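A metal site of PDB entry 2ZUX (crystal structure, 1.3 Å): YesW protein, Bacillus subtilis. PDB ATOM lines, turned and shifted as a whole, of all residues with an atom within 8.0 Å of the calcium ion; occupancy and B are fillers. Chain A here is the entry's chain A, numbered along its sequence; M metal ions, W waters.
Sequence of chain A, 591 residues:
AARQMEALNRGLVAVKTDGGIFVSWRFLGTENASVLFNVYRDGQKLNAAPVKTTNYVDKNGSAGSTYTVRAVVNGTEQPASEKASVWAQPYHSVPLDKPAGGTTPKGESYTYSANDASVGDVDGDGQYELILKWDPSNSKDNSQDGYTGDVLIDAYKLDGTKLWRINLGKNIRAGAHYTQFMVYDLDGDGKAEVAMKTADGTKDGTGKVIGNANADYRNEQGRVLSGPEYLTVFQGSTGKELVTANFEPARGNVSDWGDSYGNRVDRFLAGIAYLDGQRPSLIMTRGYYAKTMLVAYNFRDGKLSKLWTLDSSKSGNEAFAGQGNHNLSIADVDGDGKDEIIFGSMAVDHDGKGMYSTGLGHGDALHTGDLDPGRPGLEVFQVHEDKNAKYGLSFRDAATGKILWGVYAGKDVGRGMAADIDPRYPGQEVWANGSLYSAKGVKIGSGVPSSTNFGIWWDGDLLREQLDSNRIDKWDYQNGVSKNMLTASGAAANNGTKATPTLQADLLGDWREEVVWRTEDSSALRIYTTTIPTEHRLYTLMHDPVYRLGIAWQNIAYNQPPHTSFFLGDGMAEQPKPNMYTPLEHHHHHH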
ATOM      1  N   GLY A  11     -14.876 -17.020  13.028  1.00  0.00           N
ATOM      2  CA  GLY A  11     -14.288 -18.130  12.269  1.00  0.00           C
ATOM      3  C   GLY A  11     -14.410 -19.450  13.001  1.00  0.00           C
ATOM      4  O   GLY A  11     -13.603 -20.355  12.806  1.00  0.00           O
ATOM      5  N   VAL A  13     -15.108 -23.065  14.115  1.00  0.00           N
ATOM      6  CA  VAL A  13     -15.259 -24.346  13.417  1.00  0.00           C
ATOM      7  C   VAL A  13     -15.236 -25.479  14.439  1.00  0.00           C
ATOM      8  O   VAL A  13     -14.536 -25.390  15.460  1.00  0.00           O
ATOM      9  CB  VAL A  13     -14.150 -24.520  12.318  1.00  0.00           C
ATOM     10  CG1 VAL A  13     -12.786 -24.796  12.922  1.00  0.00           C
ATOM     11  CG2 VAL A  13     -14.522 -25.623  11.331  1.00  0.00           C
ATOM     12  N   SER A  24     -12.020 -24.832  17.003  1.00  0.00           N
ATOM     13  CA  SER A  24     -11.032 -23.751  16.928  1.00  0.00           C
ATOM     14  C   SER A  24     -11.652 -22.488  16.353  1.00  0.00           C
ATOM     15  O   SER A  24     -12.703 -22.516  15.706  1.00  0.00           O
ATOM     16  CB  SER A  24      -9.723 -24.161  16.223  1.00  0.00           C
ATOM     17  OG  SER A  24      -9.805 -24.032  14.802  1.00  0.00           O
ATOM     18  N   TRP A  25     -11.007 -21.358  16.650  1.00  0.00           N
ATOM     19  CA  TRP A  25     -11.559 -20.068  16.290  1.00  0.00           C
ATOM     20  C   TRP A  25     -10.448 -19.026  16.200  1.00  0.00           C
ATOM     21  O   TRP A  25      -9.296 -19.286  16.564  1.00  0.00           O
ATOM     22  CB  TRP A  25     -12.649 -19.627  17.282  1.00  0.00           C
ATOM     23  CG  TRP A  25     -12.187 -19.456  18.702  1.00  0.00           C
ATOM     24  CD1 TRP A  25     -11.744 -18.304  19.295  1.00  0.00           C
ATOM     25  CD2 TRP A  25     -12.099 -20.480  19.713  1.00  0.00           C
ATOM     26  NE1 TRP A  25     -11.407 -18.544  20.616  1.00  0.00           N
ATOM     27  CE2 TRP A  25     -11.623 -19.871  20.898  1.00  0.00           C
ATOM     28  CE3 TRP A  25     -12.392 -21.847  19.730  1.00  0.00           C
ATOM     29  CZ2 TRP A  25     -11.411 -20.582  22.084  1.00  0.00           C
ATOM     30  CZ3 TRP A  25     -12.194 -22.559  20.920  1.00  0.00           C
ATOM     31  CH2 TRP A  25     -11.706 -21.929  22.076  1.00  0.00           C
ATOM     32  N   ARG A  26     -10.805 -17.844  15.711  1.00  0.00           N
ATOM     33  CA  ARG A  26      -9.836 -16.772  15.485  1.00  0.00           C
ATOM     34  C   ARG A  26      -9.547 -15.967  16.721  1.00  0.00           C
ATOM     35  O   ARG A  26     -10.443 -15.685  17.531  1.00  0.00           O
ATOM     36  CB  ARG A  26     -10.368 -15.810  14.430  1.00  0.00           C
ATOM     37  CG  ARG A  26     -10.534 -16.404  13.053  1.00  0.00           C
ATOM     38  CD  ARG A  26     -11.327 -15.468  12.175  1.00  0.00           C
ATOM     39  NE  ARG A  26     -11.304 -15.893  10.789  1.00  0.00           N
ATOM     40  CZ  ARG A  26     -12.290 -15.697   9.917  1.00  0.00           C
ATOM     41  NH1 ARG A  26     -13.439 -15.123  10.270  1.00  0.00           N
ATOM     42  NH2 ARG A  26     -12.135 -16.109   8.664  1.00  0.00           N
ATOM     43  N   TRP A 457       1.537 -24.137   7.989  1.00  0.00           N
ATOM     44  CA  TRP A 457       1.393 -24.359   9.435  1.00  0.00           C
ATOM     45  C   TRP A 457       0.200 -25.258   9.660  1.00  0.00           C
ATOM     46  O   TRP A 457      -0.939 -24.834   9.496  1.00  0.00           O
ATOM     47  CB  TRP A 457       1.252 -23.035  10.204  1.00  0.00           C
ATOM     48  CG  TRP A 457       2.531 -22.238  10.178  1.00  0.00           C
ATOM     49  CD1 TRP A 457       3.714 -22.584  10.788  1.00  0.00           C
ATOM     50  CD2 TRP A 457       2.766 -20.996   9.508  1.00  0.00           C
ATOM     51  NE1 TRP A 457       4.676 -21.626  10.523  1.00  0.00           N
ATOM     52  CE2 TRP A 457       4.126 -20.649   9.735  1.00  0.00           C
ATOM     53  CE3 TRP A 457       1.976 -20.149   8.715  1.00  0.00           C
ATOM     54  CZ2 TRP A 457       4.691 -19.485   9.220  1.00  0.00           C
ATOM     55  CZ3 TRP A 457       2.549 -18.980   8.203  1.00  0.00           C
ATOM     56  CH2 TRP A 457       3.901 -18.675   8.445  1.00  0.00           C
ATOM     57  N   TRP A 458       0.477 -26.521  10.006  1.00  0.00           N
ATOM     58  CA  TRP A 458      -0.574 -27.544  10.100  1.00  0.00           C
ATOM     59  C   TRP A 458      -0.702 -28.202  11.462  1.00  0.00           C
ATOM     60  O   TRP A 458      -1.822 -28.383  11.950  1.00  0.00           O
ATOM     61  CB  TRP A 458      -0.350 -28.619   9.028  1.00  0.00           C
ATOM     62  CG  TRP A 458      -1.429 -29.647   9.017  1.00  0.00           C
ATOM     63  CD1 TRP A 458      -1.332 -30.943   9.440  1.00  0.00           C
ATOM     64  CD2 TRP A 458      -2.775 -29.473   8.566  1.00  0.00           C
ATOM     65  NE1 TRP A 458      -2.537 -31.588   9.258  1.00  0.00           N
ATOM     66  CE2 TRP A 458      -3.443 -30.703   8.733  1.00  0.00           C
ATOM     67  CE3 TRP A 458      -3.490 -28.390   8.018  1.00  0.00           C
ATOM     68  CZ2 TRP A 458      -4.788 -30.889   8.371  1.00  0.00           C
ATOM     69  CZ3 TRP A 458      -4.824 -28.580   7.665  1.00  0.00           C
ATOM     70  CH2 TRP A 458      -5.447 -29.820   7.854  1.00  0.00           C
ATOM     71  N   ALA A 505      -4.728 -21.255   2.987  1.00  0.00           N
ATOM     72  CA  ALA A 505      -4.916 -19.994   3.717  1.00  0.00           C
ATOM     73  C   ALA A 505      -5.520 -20.295   5.064  1.00  0.00           C
ATOM     74  O   ALA A 505      -6.340 -21.217   5.198  1.00  0.00           O
ATOM     75  CB  ALA A 505      -5.838 -19.056   2.947  1.00  0.00           C
ATOM     76  N   ASP A 506      -5.168 -19.491   6.056  1.00  0.00           N
ATOM     77  CA  ASP A 506      -5.917 -19.505   7.320  1.00  0.00           C
ATOM     78  C   ASP A 506      -7.256 -18.808   7.108  1.00  0.00           C
ATOM     79  O   ASP A 506      -7.382 -17.592   7.290  1.00  0.00           O
ATOM     80  CB  ASP A 506      -5.141 -18.799   8.436  1.00  0.00           C
ATOM     81  CG  ASP A 506      -5.944 -18.697   9.710  1.00  0.00           C
ATOM     82  OD1 ASP A 506      -6.896 -19.482   9.896  1.00  0.00           O
ATOM     83  OD2 ASP A 506      -5.610 -17.820  10.524  1.00  0.00           O
ATOM     84  N   LEU A 507      -8.260 -19.591   6.699  1.00  0.00           N
ATOM     85  CA  LEU A 507      -9.549 -19.010   6.369  1.00  0.00           C
ATOM     86  C   LEU A 507     -10.647 -19.252   7.397  1.00  0.00           C
ATOM     87  O   LEU A 507     -11.701 -18.640   7.313  1.00  0.00           O
ATOM     88  CB  LEU A 507     -10.008 -19.389   4.951  1.00  0.00           C
ATOM     89  CG  LEU A 507      -9.883 -20.808   4.414  1.00  0.00           C
ATOM     90  CD1 LEU A 507     -10.884 -21.736   5.067  1.00  0.00           C
ATOM     91  CD2 LEU A 507     -10.079 -20.823   2.899  1.00  0.00           C
ATOM     92  N   LEU A 508     -10.403 -20.145   8.356  1.00  0.00           N
ATOM     93  CA  LEU A 508     -11.322 -20.363   9.478  1.00  0.00           C
ATOM     94  C   LEU A 508     -10.548 -20.945  10.649  1.00  0.00           C
ATOM     95  O   LEU A 508      -9.396 -21.336  10.492  1.00  0.00           O
ATOM     96  CB  LEU A 508     -12.512 -21.248   9.099  1.00  0.00           C
ATOM     97  CG  LEU A 508     -12.271 -22.560   8.365  1.00  0.00           C
ATOM     98  CD1 LEU A 508     -11.883 -23.675   9.323  1.00  0.00           C
ATOM     99  CD2 LEU A 508     -13.529 -22.949   7.577  1.00  0.00           C
ATOM    100  N   GLY A 509     -11.161 -20.968  11.826  1.00  0.00           N
ATOM    101  CA  GLY A 509     -10.524 -21.557  12.986  1.00  0.00           C
ATOM    102  C   GLY A 509      -9.333 -20.749  13.469  1.00  0.00           C
ATOM    103  O   GLY A 509      -9.233 -19.555  13.201  1.00  0.00           O
ATOM    104  N   ASP A 510      -8.428 -21.435  14.180  1.00  0.00           N
ATOM    105  CA  ASP A 510      -7.240 -20.783  14.725  1.00  0.00           C
ATOM    106  C   ASP A 510      -6.161 -20.582  13.680  1.00  0.00           C
ATOM    107  O   ASP A 510      -6.384 -20.783  12.486  1.00  0.00           O
ATOM    108  CB  ASP A 510      -6.732 -21.521  15.991  1.00  0.00           C
ATOM    109  CG  ASP A 510      -6.087 -22.876  15.691  1.00  0.00           C
ATOM    110  OD1 ASP A 510      -5.746 -23.180  14.522  1.00  0.00           O
ATOM    111  OD2 ASP A 510      -5.867 -23.627  16.668  1.00  0.00           O
ATOM    112  N   TRP A 511      -4.973 -20.200  14.138  1.00  0.00           N
ATOM    113  CA  TRP A 511      -3.924 -19.703  13.250  1.00  0.00           C
ATOM    114  C   TRP A 511      -3.368 -20.692  12.227  1.00  0.00           C
ATOM    115  O   TRP A 511      -2.714 -20.267  11.280  1.00  0.00           O
ATOM    116  CB  TRP A 511      -2.774 -19.118  14.077  1.00  0.00           C
ATOM    117  CG  TRP A 511      -2.055 -20.119  14.925  1.00  0.00           C
ATOM    118  CD1 TRP A 511      -2.423 -20.544  16.180  1.00  0.00           C
ATOM    119  CD2 TRP A 511      -0.842 -20.821  14.613  1.00  0.00           C
ATOM    120  NE1 TRP A 511      -1.519 -21.470  16.645  1.00  0.00           N
ATOM    121  CE2 TRP A 511      -0.545 -21.663  15.700  1.00  0.00           C
ATOM    122  CE3 TRP A 511       0.015 -20.828  13.497  1.00  0.00           C
ATOM    123  CZ2 TRP A 511       0.585 -22.488  15.732  1.00  0.00           C
ATOM    124  CZ3 TRP A 511       1.145 -21.652  13.529  1.00  0.00           C
ATOM    125  CH2 TRP A 511       1.410 -22.468  14.632  1.00  0.00           C
ATOM    126  N   ARG A 512      -3.628 -21.992  12.402  1.00  0.00           N
ATOM    127  CA  ARG A 512      -3.134 -22.931  11.404  1.00  0.00           C
ATOM    128  C   ARG A 512      -3.842 -22.705  10.065  1.00  0.00           C
ATOM    129  O   ARG A 512      -4.949 -22.173  10.011  1.00  0.00           O
ATOM    130  CB  ARG A 512      -3.261 -24.381  11.872  1.00  0.00           C
ATOM    131  CG  ARG A 512      -2.087 -24.870  12.729  1.00  0.00           C
ATOM    132  CD  ARG A 512      -2.128 -24.339  14.168  1.00  0.00           C
ATOM    133  NE  ARG A 512      -3.331 -24.725  14.899  1.00  0.00           N
ATOM    134  CZ  ARG A 512      -3.530 -25.909  15.459  1.00  0.00           C
ATOM    135  NH1 ARG A 512      -4.670 -26.148  16.106  1.00  0.00           N
ATOM    136  NH2 ARG A 512      -2.617 -26.870  15.376  1.00  0.00           N
ATOM    137  N   GLU A 513      -3.165 -23.088   8.976  1.00  0.00           N
ATOM    138  CA  GLU A 513      -3.691 -22.853   7.650  1.00  0.00           C
ATOM    139  C   GLU A 513      -4.585 -23.994   7.179  1.00  0.00           C
ATOM    140  O   GLU A 513      -4.280 -25.153   7.375  1.00  0.00           O
ATOM    141  CB  GLU A 513      -2.532 -22.661   6.687  1.00  0.00           C
ATOM    142  CG  GLU A 513      -1.625 -21.507   7.081  1.00  0.00           C
ATOM    143  CD  GLU A 513      -0.460 -21.339   6.135  1.00  0.00           C
ATOM    144  OE1 GLU A 513       0.593 -21.968   6.396  1.00  0.00           O
ATOM    145  OE2 GLU A 513      -0.615 -20.617   5.126  1.00  0.00           O
ATOM    146  N   GLU A 514      -5.709 -23.634   6.550  1.00  0.00           N
ATOM    147  CA  GLU A 514      -6.590 -24.598   5.896  1.00  0.00           C
ATOM    148  C   GLU A 514      -6.065 -24.873   4.497  1.00  0.00           C
ATOM    149  O   GLU A 514      -5.305 -24.075   3.929  1.00  0.00           O
ATOM    150  CB  GLU A 514      -8.008 -24.065   5.803  1.00  0.00           C
ATOM    151  CG  GLU A 514      -8.795 -24.084   7.110  1.00  0.00           C
ATOM    152  CD  GLU A 514      -8.151 -23.267   8.225  1.00  0.00           C
ATOM    153  OE1 GLU A 514      -7.915 -22.045   8.034  1.00  0.00           O
ATOM    154  OE2 GLU A 514      -7.869 -23.848   9.301  1.00  0.00           O
ATOM    155  N   VAL A 515      -6.454 -26.027   3.953  1.00  0.00           N
ATOM    156  CA  VAL A 515      -6.160 -26.353   2.568  1.00  0.00           C
ATOM    157  C   VAL A 515      -7.452 -26.606   1.832  1.00  0.00           C
ATOM    158  O   VAL A 515      -8.335 -27.323   2.330  1.00  0.00           O
ATOM    159  CB  VAL A 515      -5.275 -27.598   2.425  1.00  0.00           C
ATOM    160  CG1 VAL A 515      -4.806 -27.741   0.988  1.00  0.00           C
ATOM    161  CG2 VAL A 515      -4.103 -27.540   3.361  1.00  0.00           C
ATOM    162  N   TYR A 528      -9.931 -28.592   4.214  1.00  0.00           N
ATOM    163  CA  TYR A 528      -9.360 -29.311   5.355  1.00  0.00           C
ATOM    164  C   TYR A 528      -8.884 -28.305   6.395  1.00  0.00           C
ATOM    165  O   TYR A 528      -8.193 -27.348   6.054  1.00  0.00           O
ATOM    166  CB  TYR A 528      -8.178 -30.165   4.904  1.00  0.00           C
ATOM    167  CG  TYR A 528      -8.555 -31.375   4.071  1.00  0.00           C
ATOM    168  CD1 TYR A 528      -8.533 -32.658   4.634  1.00  0.00           C
ATOM    169  CD2 TYR A 528      -8.934 -31.251   2.742  1.00  0.00           C
ATOM    170  CE1 TYR A 528      -8.882 -33.773   3.877  1.00  0.00           C
ATOM    171  CE2 TYR A 528      -9.279 -32.370   1.977  1.00  0.00           C
ATOM    172  CZ  TYR A 528      -9.246 -33.616   2.554  1.00  0.00           C
ATOM    173  OH  TYR A 528      -9.600 -34.715   1.785  1.00  0.00           O
ATOM    174  N   THR A 529      -9.278 -28.518   7.643  1.00  0.00           N
ATOM    175  CA  THR A 529      -8.796 -27.716   8.763  1.00  0.00           C
ATOM    176  C   THR A 529      -8.157 -28.677   9.758  1.00  0.00           C
ATOM    177  O   THR A 529      -8.639 -29.796   9.942  1.00  0.00           O
ATOM    178  CB  THR A 529      -9.922 -26.864   9.409  1.00  0.00           C
ATOM    179  OG1 THR A 529      -9.347 -25.865  10.271  1.00  0.00           O
ATOM    180  CG2 THR A 529     -10.910 -27.714  10.227  1.00  0.00           C
ATOM    181  N   THR A 530      -7.074 -28.259  10.402  1.00  0.00           N
ATOM    182  CA  THR A 530      -6.383 -29.147  11.319  1.00  0.00           C
ATOM    183  C   THR A 530      -7.202 -29.430  12.579  1.00  0.00           C
ATOM    184  O   THR A 530      -7.947 -28.567  13.070  1.00  0.00           O
ATOM    185  CB  THR A 530      -4.982 -28.615  11.676  1.00  0.00           C
ATOM    186  OG1 THR A 530      -4.239 -29.668  12.292  1.00  0.00           O
ATOM    187  CG2 THR A 530      -5.041 -27.426  12.632  1.00  0.00           C
ATOM    188  N   THR A 540      -5.179 -14.225  13.796  1.00  0.00           N
ATOM    189  CA  THR A 540      -5.515 -14.823  12.517  1.00  0.00           C
ATOM    190  C   THR A 540      -4.581 -14.287  11.441  1.00  0.00           C
ATOM    191  O   THR A 540      -4.282 -13.087  11.394  1.00  0.00           O
ATOM    192  CB  THR A 540      -7.001 -14.624  12.141  1.00  0.00           C
ATOM    193  OG1 THR A 540      -7.245 -15.242  10.869  1.00  0.00           O
ATOM    194  CG2 THR A 540      -7.387 -13.146  12.046  1.00  0.00           C
ATOM    195  N   LEU A 541      -4.076 -15.181  10.597  1.00  0.00           N
ATOM    196  CA  LEU A 541      -3.041 -14.790   9.648  1.00  0.00           C
ATOM    197  C   LEU A 541      -3.550 -13.807   8.598  1.00  0.00           C
ATOM    198  O   LEU A 541      -2.779 -13.038   8.039  1.00  0.00           O
ATOM    199  CB  LEU A 541      -2.408 -16.030   9.009  1.00  0.00           C
ATOM    200  CG  LEU A 541      -1.872 -17.089   9.973  1.00  0.00           C
ATOM    201  CD1 LEU A 541      -1.199 -18.213   9.199  1.00  0.00           C
ATOM    202  CD2 LEU A 541      -0.908 -16.473  11.011  1.00  0.00           C
ATOM    203  N   TYR A 547       0.928 -11.634   5.023  1.00  0.00           N
ATOM    204  CA  TYR A 547       0.228 -12.872   4.770  1.00  0.00           C
ATOM    205  C   TYR A 547      -1.047 -12.629   3.955  1.00  0.00           C
ATOM    206  O   TYR A 547      -1.320 -13.331   2.991  1.00  0.00           O
ATOM    207  CB  TYR A 547      -0.099 -13.593   6.082  1.00  0.00           C
ATOM    208  CG  TYR A 547      -0.685 -14.974   5.885  1.00  0.00           C
ATOM    209  CD1 TYR A 547       0.113 -16.101   5.950  1.00  0.00           C
ATOM    210  CD2 TYR A 547      -2.041 -15.128   5.630  1.00  0.00           C
ATOM    211  CE1 TYR A 547      -0.432 -17.381   5.757  1.00  0.00           C
ATOM    212  CE2 TYR A 547      -2.601 -16.384   5.440  1.00  0.00           C
ATOM    213  CZ  TYR A 547      -1.793 -17.490   5.515  1.00  0.00           C
ATOM    214  OH  TYR A 547      -2.378 -18.719   5.321  1.00  0.00           O
HETATM  215 CA    CA M   1      -7.157 -21.797  10.511  1.00  0.00          CA
HETATM  216  O   HOH W   1      -7.079 -23.550  12.203  1.00  0.00           O
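Gly 509 touches the calcium ion.
NH1 of Arg 512 is in salt-bridge range of OD2 of Asp 510, at 2.8 Å. The backbone NH (N) of Asp 510 is in hydrogen-bond range of the side-chain hydroxyl (OG) of Ser 24 (3.0 Å). N of Asp 510 sits close to O of Trp 25 (3.3 Å). OG1 of Thr 540 is in hydrogen-bond range of OD2 of Asp 506 (3.1 Å). The backbone NH of Asp 506 lies within hydrogen-bond range of the side-chain hydroxyl of Tyr 547 (3.0 Å). The side-chain carboxylate of Glu 514 lies close to the backbone NH of Leu 507. The side-chain hydroxyl (OG1) of Thr 529 lies close to the side-chain carboxylate (OE2) of Glu 514. The backbone carbonyl oxygen (O) of Gly 509 lies close to the backbone NH (N) of Arg 26 (3.4 Å).
The calcium ion is bound by the backbone carbonyl oxygen (O) of Leu 508, the backbone carbonyl oxygen (O) of Arg 512, the backbone carbonyl oxygen (O) of Asp 510, the side-chain carboxylate (OD1) of Asp 506, water W1, the side-chain carboxylate (OE2) of Glu 514 and the side-chain carboxylate (OE1) of Glu 514.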
